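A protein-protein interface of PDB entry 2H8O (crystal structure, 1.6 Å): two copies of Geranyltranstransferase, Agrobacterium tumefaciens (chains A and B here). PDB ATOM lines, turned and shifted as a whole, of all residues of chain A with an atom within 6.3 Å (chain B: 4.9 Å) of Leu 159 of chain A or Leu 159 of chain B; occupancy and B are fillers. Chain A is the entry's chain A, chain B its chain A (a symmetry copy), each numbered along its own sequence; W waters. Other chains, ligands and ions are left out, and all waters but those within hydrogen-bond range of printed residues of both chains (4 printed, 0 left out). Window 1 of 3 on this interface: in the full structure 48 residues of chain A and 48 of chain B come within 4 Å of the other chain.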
ATOM      1  N   CYS A 116     -15.474  16.537 -16.668  1.00  0.00           N
ATOM      2  CA  CYS A 116     -15.431  17.954 -17.017  1.00  0.00           C
ATOM      3  C   CYS A 116     -14.526  18.150 -18.227  1.00  0.00           C
ATOM      4  O   CYS A 116     -14.848  18.878 -19.142  1.00  0.00           O
ATOM      5  CB  CYS A 116     -14.899  18.813 -15.877  1.00  0.00           C
ATOM      6  SG  CYS A 116     -16.106  19.115 -14.591  1.00  0.00           S
ATOM      7  N   LEU A 117     -13.368  17.477 -18.219  1.00  0.00           N
ATOM      8  CA  LEU A 117     -12.426  17.619 -19.334  1.00  0.00           C
ATOM      9  C   LEU A 117     -13.039  17.025 -20.619  1.00  0.00           C
ATOM     10  O   LEU A 117     -12.993  17.646 -21.687  1.00  0.00           O
ATOM     11  CB  LEU A 117     -11.075  17.000 -18.957  1.00  0.00           C
ATOM     12  CG  LEU A 117      -9.898  17.451 -19.849  1.00  0.00           C
ATOM     13  CD1 LEU A 117      -8.561  17.470 -19.094  1.00  0.00           C
ATOM     14  CD2 LEU A 117      -9.858  16.630 -21.106  1.00  0.00           C
ATOM     15  N   TYR A 120     -15.526  19.491 -21.913  1.00  0.00           N
ATOM     16  CA  TYR A 120     -14.933  20.692 -22.501  1.00  0.00           C
ATOM     17  C   TYR A 120     -14.568  20.393 -23.942  1.00  0.00           C
ATOM     18  O   TYR A 120     -14.737  21.238 -24.833  1.00  0.00           O
ATOM     19  CB  TYR A 120     -13.695  21.184 -21.712  1.00  0.00           C
ATOM     20  CG  TYR A 120     -12.360  21.113 -22.474  1.00  0.00           C
ATOM     21  CD1 TYR A 120     -12.050  22.022 -23.474  1.00  0.00           C
ATOM     22  CD2 TYR A 120     -11.404  20.163 -22.133  1.00  0.00           C
ATOM     23  CE1 TYR A 120     -10.854  21.965 -24.166  1.00  0.00           C
ATOM     24  CE2 TYR A 120     -10.209  20.091 -22.811  1.00  0.00           C
ATOM     25  CZ  TYR A 120      -9.923  20.999 -23.817  1.00  0.00           C
ATOM     26  OH  TYR A 120      -8.720  20.972 -24.527  1.00  0.00           O
ATOM     27  N   ALA A 154     -16.618  28.568 -21.801  1.00  0.00           N
ATOM     28  CA  ALA A 154     -17.179  27.445 -21.020  1.00  0.00           C
ATOM     29  C   ALA A 154     -16.263  26.236 -21.112  1.00  0.00           C
ATOM     30  O   ALA A 154     -15.961  25.591 -20.120  1.00  0.00           O
ATOM     31  CB  ALA A 154     -18.606  27.071 -21.501  1.00  0.00           C
ATOM     32  N   GLY A 155     -15.786  25.948 -22.317  1.00  0.00           N
ATOM     33  CA  GLY A 155     -14.830  24.860 -22.463  1.00  0.00           C
ATOM     34  C   GLY A 155     -13.534  25.151 -21.725  1.00  0.00           C
ATOM     35  O   GLY A 155     -12.983  24.291 -21.058  1.00  0.00           O
ATOM     36  N   ASP A 156     -13.050  26.386 -21.841  1.00  0.00           N
ATOM     37  CA  ASP A 156     -11.813  26.792 -21.165  1.00  0.00           C
ATOM     38  C   ASP A 156     -11.970  26.610 -19.648  1.00  0.00           C
ATOM     39  O   ASP A 156     -11.075  26.135 -18.940  1.00  0.00           O
ATOM     40  CB  ASP A 156     -11.460  28.265 -21.473  1.00  0.00           C
ATOM     41  CG  ASP A 156     -10.980  28.475 -22.897  1.00  0.00           C
ATOM     42  OD1 ASP A 156     -10.734  27.472 -23.605  1.00  0.00           O
ATOM     43  OD2 ASP A 156     -10.871  29.668 -23.329  1.00  0.00           O
ATOM     44  N   SER A 157     -13.142  26.994 -19.158  1.00  0.00           N
ATOM     45  CA  SER A 157     -13.413  26.947 -17.725  1.00  0.00           C
ATOM     46  C   SER A 157     -13.572  25.496 -17.231  1.00  0.00           C
ATOM     47  O   SER A 157     -13.159  25.161 -16.138  1.00  0.00           O
ATOM     48  CB  SER A 157     -14.620  27.787 -17.351  1.00  0.00           C
ATOM     49  OG  SER A 157     -14.453  29.165 -17.704  1.00  0.00           O
ATOM     50  N   LEU A 158     -14.185  24.638 -18.047  1.00  0.00           N
ATOM     51  CA  LEU A 158     -14.318  23.208 -17.698  1.00  0.00           C
ATOM     52  C   LEU A 158     -12.961  22.504 -17.694  1.00  0.00           C
ATOM     53  O   LEU A 158     -12.700  21.672 -16.831  1.00  0.00           O
ATOM     54  CB  LEU A 158     -15.275  22.512 -18.660  1.00  0.00           C
ATOM     55  CG  LEU A 158     -16.760  22.772 -18.416  1.00  0.00           C
ATOM     56  CD1 LEU A 158     -17.549  22.241 -19.665  1.00  0.00           C
ATOM     57  CD2 LEU A 158     -17.266  22.121 -17.142  1.00  0.00           C
ATOM     58  N   LEU A 159     -12.097  22.840 -18.666  1.00  0.00           N
ATOM     59  CA  LEU A 159     -10.726  22.295 -18.673  1.00  0.00           C
ATOM     60  C   LEU A 159      -9.970  22.724 -17.393  1.00  0.00           C
ATOM     61  O   LEU A 159      -9.320  21.915 -16.739  1.00  0.00           O
ATOM     62  CB  LEU A 159      -9.999  22.741 -19.934  1.00  0.00           C
ATOM     63  CG  LEU A 159      -8.512  22.466 -20.015  1.00  0.00           C
ATOM     64  CD1 LEU A 159      -8.191  21.000 -19.732  1.00  0.00           C
ATOM     65  CD2 LEU A 159      -7.980  22.857 -21.395  1.00  0.00           C
ATOM     66  N   THR A 160     -10.078  24.007 -17.048  1.00  0.00           N
ATOM     67  CA  THR A 160      -9.429  24.563 -15.868  1.00  0.00           C
ATOM     68  C   THR A 160      -9.964  23.867 -14.600  1.00  0.00           C
ATOM     69  O   THR A 160      -9.215  23.492 -13.710  1.00  0.00           O
ATOM     70  CB  THR A 160      -9.631  26.081 -15.782  1.00  0.00           C
ATOM     71  OG1 THR A 160      -9.207  26.690 -17.018  1.00  0.00           O
ATOM     72  CG2 THR A 160      -8.817  26.673 -14.627  1.00  0.00           C
ATOM     73  N   LEU A 161     -11.285  23.741 -14.529  1.00  0.00           N
ATOM     74  CA  LEU A 161     -11.945  23.134 -13.355  1.00  0.00           C
ATOM     75  C   LEU A 161     -11.523  21.681 -13.124  1.00  0.00           C
ATOM     76  O   LEU A 161     -11.436  21.221 -11.963  1.00  0.00           O
ATOM     77  CB  LEU A 161     -13.478  23.219 -13.503  1.00  0.00           C
ATOM     78  CG  LEU A 161     -14.242  23.022 -12.186  1.00  0.00           C
ATOM     79  CD1 LEU A 161     -14.012  24.218 -11.274  1.00  0.00           C
ATOM     80  CD2 LEU A 161     -15.700  22.827 -12.495  1.00  0.00           C
ATOM     81  N   ALA A 162     -11.271  20.933 -14.201  1.00  0.00           N
ATOM     82  CA  ALA A 162     -10.807  19.545 -14.077  1.00  0.00           C
ATOM     83  C   ALA A 162      -9.592  19.467 -13.153  1.00  0.00           C
ATOM     84  O   ALA A 162      -9.496  18.600 -12.283  1.00  0.00           O
ATOM     85  CB  ALA A 162     -10.503  18.952 -15.444  1.00  0.00           C
ATOM     86  N   PHE A 163      -8.649  20.388 -13.336  1.00  0.00           N
ATOM     87  CA  PHE A 163      -7.436  20.400 -12.523  1.00  0.00           C
ATOM     88  C   PHE A 163      -7.678  20.836 -11.082  1.00  0.00           C
ATOM     89  O   PHE A 163      -7.136  20.234 -10.155  1.00  0.00           O
ATOM     90  CB  PHE A 163      -6.334  21.182 -13.225  1.00  0.00           C
ATOM     91  CG  PHE A 163      -5.854  20.488 -14.457  1.00  0.00           C
ATOM     92  CD1 PHE A 163      -5.042  19.387 -14.336  1.00  0.00           C
ATOM     93  CD2 PHE A 163      -6.296  20.860 -15.724  1.00  0.00           C
ATOM     94  CE1 PHE A 163      -4.592  18.711 -15.469  1.00  0.00           C
ATOM     95  CE2 PHE A 163      -5.866  20.186 -16.837  1.00  0.00           C
ATOM     96  CZ  PHE A 163      -5.027  19.114 -16.715  1.00  0.00           C
ATOM     97  N   ASP A 164      -8.542  21.838 -10.911  1.00  0.00           N
ATOM     98  CA  ASP A 164      -9.028  22.205  -9.580  1.00  0.00           C
ATOM     99  C   ASP A 164      -9.622  21.003  -8.838  1.00  0.00           C
ATOM    100  O   ASP A 164      -9.293  20.756  -7.697  1.00  0.00           O
ATOM    101  CB  ASP A 164     -10.067  23.329  -9.697  1.00  0.00           C
ATOM    102  CG  ASP A 164     -10.449  23.943  -8.359  1.00  0.00           C
ATOM    103  OD1 ASP A 164      -9.767  23.713  -7.338  1.00  0.00           O
ATOM    104  OD2 ASP A 164     -11.451  24.696  -8.331  1.00  0.00           O
ATOM    105  N   ALA A 189      -4.309  14.733 -22.181  1.00  0.00           N
ATOM    106  CA  ALA A 189      -5.262  15.704 -22.726  1.00  0.00           C
ATOM    107  C   ALA A 189      -4.696  16.728 -23.719  1.00  0.00           C
ATOM    108  O   ALA A 189      -5.455  17.317 -24.507  1.00  0.00           O
ATOM    109  CB  ALA A 189      -5.933  16.439 -21.570  1.00  0.00           C
ATOM    110  N   CYS B 116       2.553  30.287 -19.993  1.00  0.00           N
ATOM    111  CA  CYS B 116       1.799  29.486 -20.953  1.00  0.00           C
ATOM    112  C   CYS B 116       0.313  29.793 -20.811  1.00  0.00           C
ATOM    113  O   CYS B 116      -0.391  29.954 -21.786  1.00  0.00           O
ATOM    114  CB  CYS B 116       2.001  27.991 -20.741  1.00  0.00           C
ATOM    115  SG  CYS B 116       3.558  27.387 -21.384  1.00  0.00           S
ATOM    116  N   LEU B 117      -0.161  29.874 -19.562  1.00  0.00           N
ATOM    117  CA  LEU B 117      -1.583  30.148 -19.330  1.00  0.00           C
ATOM    118  C   LEU B 117      -1.930  31.573 -19.810  1.00  0.00           C
ATOM    119  O   LEU B 117      -2.932  31.781 -20.502  1.00  0.00           O
ATOM    120  CB  LEU B 117      -1.930  29.897 -17.857  1.00  0.00           C
ATOM    121  CG  LEU B 117      -3.439  29.734 -17.578  1.00  0.00           C
ATOM    122  CD1 LEU B 117      -3.721  28.802 -16.392  1.00  0.00           C
ATOM    123  CD2 LEU B 117      -4.088  31.082 -17.441  1.00  0.00           C
ATOM    124  N   TYR B 120      -2.169  31.469 -23.535  1.00  0.00           N
ATOM    125  CA  TYR B 120      -3.358  30.783 -24.043  1.00  0.00           C
ATOM    126  C   TYR B 120      -4.512  31.765 -24.054  1.00  0.00           C
ATOM    127  O   TYR B 120      -5.333  31.778 -24.983  1.00  0.00           O
ATOM    128  CB  TYR B 120      -3.714  29.528 -23.209  1.00  0.00           C
ATOM    129  CG  TYR B 120      -5.052  29.600 -22.451  1.00  0.00           C
ATOM    130  CD1 TYR B 120      -6.264  29.473 -23.112  1.00  0.00           C
ATOM    131  CD2 TYR B 120      -5.071  29.740 -21.068  1.00  0.00           C
ATOM    132  CE1 TYR B 120      -7.471  29.539 -22.440  1.00  0.00           C
ATOM    133  CE2 TYR B 120      -6.262  29.808 -20.383  1.00  0.00           C
ATOM    134  CZ  TYR B 120      -7.464  29.692 -21.062  1.00  0.00           C
ATOM    135  OH  TYR B 120      -8.697  29.747 -20.409  1.00  0.00           O
ATOM    136  N   GLY B 155      -4.478  27.235 -27.856  1.00  0.00           N
ATOM    137  CA  GLY B 155      -4.799  27.774 -26.543  1.00  0.00           C
ATOM    138  C   GLY B 155      -5.160  26.673 -25.559  1.00  0.00           C
ATOM    139  O   GLY B 155      -4.728  26.682 -24.419  1.00  0.00           O
ATOM    140  N   ASP B 156      -5.955  25.707 -26.016  1.00  0.00           N
ATOM    141  CA  ASP B 156      -6.363  24.583 -25.166  1.00  0.00           C
ATOM    142  C   ASP B 156      -5.118  23.824 -24.682  1.00  0.00           C
ATOM    143  O   ASP B 156      -4.997  23.419 -23.521  1.00  0.00           O
ATOM    144  CB  ASP B 156      -7.295  23.613 -25.925  1.00  0.00           C
ATOM    145  CG  ASP B 156      -8.679  24.186 -26.166  1.00  0.00           C
ATOM    146  OD1 ASP B 156      -8.999  25.252 -25.592  1.00  0.00           O
ATOM    147  OD2 ASP B 156      -9.459  23.572 -26.966  1.00  0.00           O
ATOM    148  N   SER B 157      -4.181  23.643 -25.604  1.00  0.00           N
ATOM    149  CA  SER B 157      -2.973  22.878 -25.313  1.00  0.00           C
ATOM    150  C   SER B 157      -2.033  23.653 -24.369  1.00  0.00           C
ATOM    151  O   SER B 157      -1.389  23.072 -23.517  1.00  0.00           O
ATOM    152  CB  SER B 157      -2.251  22.458 -26.580  1.00  0.00           C
ATOM    153  OG  SER B 157      -3.070  21.646 -27.427  1.00  0.00           O
ATOM    154  N   LEU B 158      -1.954  24.974 -24.536  1.00  0.00           N
ATOM    155  CA  LEU B 158      -1.140  25.814 -23.633  1.00  0.00           C
ATOM    156  C   LEU B 158      -1.729  25.852 -22.222  1.00  0.00           C
ATOM    157  O   LEU B 158      -0.989  25.818 -21.244  1.00  0.00           O
ATOM    158  CB  LEU B 158      -1.010  27.226 -24.193  1.00  0.00           C
ATOM    159  CG  LEU B 158      -0.016  27.391 -25.340  1.00  0.00           C
ATOM    160  CD1 LEU B 158      -0.251  28.808 -25.974  1.00  0.00           C
ATOM    161  CD2 LEU B 158       1.425  27.233 -24.894  1.00  0.00           C
ATOM    162  N   LEU B 159      -3.066  25.926 -22.121  1.00  0.00           N
ATOM    163  CA  LEU B 159      -3.724  25.854 -20.803  1.00  0.00           C
ATOM    164  C   LEU B 159      -3.414  24.501 -20.120  1.00  0.00           C
ATOM    165  O   LEU B 159      -3.069  24.449 -18.944  1.00  0.00           O
ATOM    166  CB  LEU B 159      -5.222  26.076 -20.960  1.00  0.00           C
ATOM    167  CG  LEU B 159      -6.096  25.819 -19.750  1.00  0.00           C
ATOM    168  CD1 LEU B 159      -5.594  26.573 -18.520  1.00  0.00           C
ATOM    169  CD2 LEU B 159      -7.541  26.219 -20.051  1.00  0.00           C
ATOM    170  N   THR B 160      -3.533  23.415 -20.883  1.00  0.00           N
ATOM    171  CA  THR B 160      -3.271  22.070 -20.387  1.00  0.00           C
ATOM    172  C   THR B 160      -1.801  21.957 -19.935  1.00  0.00           C
ATOM    173  O   THR B 160      -1.495  21.417 -18.882  1.00  0.00           O
ATOM    174  CB  THR B 160      -3.598  21.011 -21.447  1.00  0.00           C
ATOM    175  OG1 THR B 160      -4.948  21.204 -21.914  1.00  0.00           O
ATOM    176  CG2 THR B 160      -3.467  19.600 -20.863  1.00  0.00           C
ATOM    177  N   LEU B 161      -0.901  22.448 -20.780  1.00  0.00           N
ATOM    178  CA  LEU B 161       0.548  22.371 -20.502  1.00  0.00           C
ATOM    179  C   LEU B 161       0.945  23.114 -19.225  1.00  0.00           C
ATOM    180  O   LEU B 161       1.879  22.690 -18.507  1.00  0.00           O
ATOM    181  CB  LEU B 161       1.349  22.920 -21.701  1.00  0.00           C
ATOM    182  CG  LEU B 161       2.826  22.500 -21.707  1.00  0.00           C
ATOM    183  CD1 LEU B 161       2.935  21.010 -21.994  1.00  0.00           C
ATOM    184  CD2 LEU B 161       3.560  23.320 -22.729  1.00  0.00           C
ATOM    185  N   ALA B 162       0.272  24.227 -18.924  1.00  0.00           N
ATOM    186  CA  ALA B 162       0.546  24.976 -17.690  1.00  0.00           C
ATOM    187  C   ALA B 162       0.492  24.049 -16.477  1.00  0.00           C
ATOM    188  O   ALA B 162       1.349  24.090 -15.593  1.00  0.00           O
ATOM    189  CB  ALA B 162      -0.419  26.142 -17.540  1.00  0.00           C
ATOM    190  N   PHE B 163      -0.525  23.192 -16.431  1.00  0.00           N
ATOM    191  CA  PHE B 163      -0.687  22.270 -15.310  1.00  0.00           C
ATOM    192  C   PHE B 163       0.346  21.149 -15.295  1.00  0.00           C
ATOM    193  O   PHE B 163       0.882  20.817 -14.238  1.00  0.00           O
ATOM    194  CB  PHE B 163      -2.128  21.780 -15.229  1.00  0.00           C
ATOM    195  CG  PHE B 163      -3.069  22.875 -14.847  1.00  0.00           C
ATOM    196  CD1 PHE B 163      -3.107  23.305 -13.544  1.00  0.00           C
ATOM    197  CD2 PHE B 163      -3.832  23.546 -15.799  1.00  0.00           C
ATOM    198  CE1 PHE B 163      -3.966  24.335 -13.162  1.00  0.00           C
ATOM    199  CE2 PHE B 163      -4.665  24.569 -15.427  1.00  0.00           C
ATOM    200  CZ  PHE B 163      -4.729  24.970 -14.122  1.00  0.00           C
HETATM  201  O   HOH W   1     -10.208  31.809 -21.549  1.00  0.00           O
HETATM  202  O   HOH W   2      -8.540  29.386 -17.715  1.00  0.00           O
HETATM  203  O   HOH W   3      -6.764  19.502 -23.332  1.00  0.00           O
HETATM  204  O   HOH W   4      -9.310  20.728 -27.252  1.00  0.00           O
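Along chain B the printed residues that touch a printed residue of chain A span positions 120 to 163.
Hydrophobic or aromatic side chains of chain A within 4 Å of the printed part of chain B: Tyr 120, Leu 159 and Phe 163.
Among the printed residues, 9 pairs touch across the chains.
Among the printed residues, no Asp or Glu carboxylate lies within 4 Å of a Lys or Arg side-chain nitrogen of the other chain.
Water W3 lies within hydrogen-bond range of OH of Tyr 120 of chain A, O of Ala 189 of chain A and OG1 of Thr 160 of chain B.
Water W2 lies within hydrogen-bond range of the side-chain hydroxyl of Tyr 120 of chain B and the side-chain hydroxyl of Thr 160 of chain A.
Water W4 bridges the side-chain hydroxyl (OH) of Tyr 120 of chain A (2.8 Å) and the side-chain carboxylate (OD2) of Asp 156 of chain B (2.9 Å).
Water W1 lies within hydrogen-bond range of the side-chain hydroxyl (OH) of Tyr 120 of chain B and the side-chain carboxylate (OD2) of Asp 156 of chain A.
The backbone carbonyl oxygen of Asp 156 of chain B sits at hydrogen-bond distance from the side-chain hydroxyl of Thr 160 of chain B, 2.7 Å away.
O of Asp 156 of chain A is in hydrogen-bond range of OG1 of Thr 160 of chain A (2.7 Å).
Of chain B, only Asp 156, Leu 159 and Thr 160 come within 4 Å of Leu 159 of chain A.
Leu 159 of chain B touches three residues of chain A.
Of the printed residues of chain A, Thr 160 of chain B touches Leu 159.
Printed residues of chain A within 4 Å of Asp 156 of chain B: Tyr 120, Asp 156 and Leu 159.
Ala 189 of chain A touches none of the printed residues of chain B.
The nearest residue of chain A that does not touch Leu 159 of chain B is Phe 163 of chain A (5.5 Å).
Asp 156 of chain B touches Tyr 120 of chain A (CB to OH, 3.3 Å).
Tyr 120 of chain B touches Asp 156 of chain A (OH to CB, 3.3 Å).
Leu 159 of chain B touches Asp 156 of chain A.
Asp 156 of chain B touches Leu 159 of chain A (O to CD2, 3.7 Å).
Leu 159 of chain A touches Leu 159 of chain B (CD2 to CD2, 3.6 Å).
Leu 159 of chain A touches Thr 160 of chain B (CD2 to OG1, 3.5 Å).
Leu 159 of chain B touches Thr 160 of chain A (CD2 to OG1, 3.5 Å).
CD2 of Phe 163 of chain A touches CD2 of Phe 163 of chain B (3.6 Å).
Tyr 120 of chain A touches Asp 156 of chain B, and with the chains exchanged Asp 156 of chain A touches Tyr 120 of chain B.
Asp 156 of chain A touches its own counterpart, Asp 156 of chain B.
Leu 159 of chain A touches its own counterpart, Leu 159 of chain B.
Leu 159 of chain A touches Thr 160 of chain B, and with the chains exchanged Thr 160 of chain A touches Leu 159 of chain B.
12 positions are printed for both chains.
Of the 9 pairs that touch across the chains among the printed residues, 9 have their exchanged pair printed and touching as well.
The side-chain carboxylate of Asp 156 of chain A sits close to the side-chain carboxylate of Asp 156 of chain B (3.4 Å).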
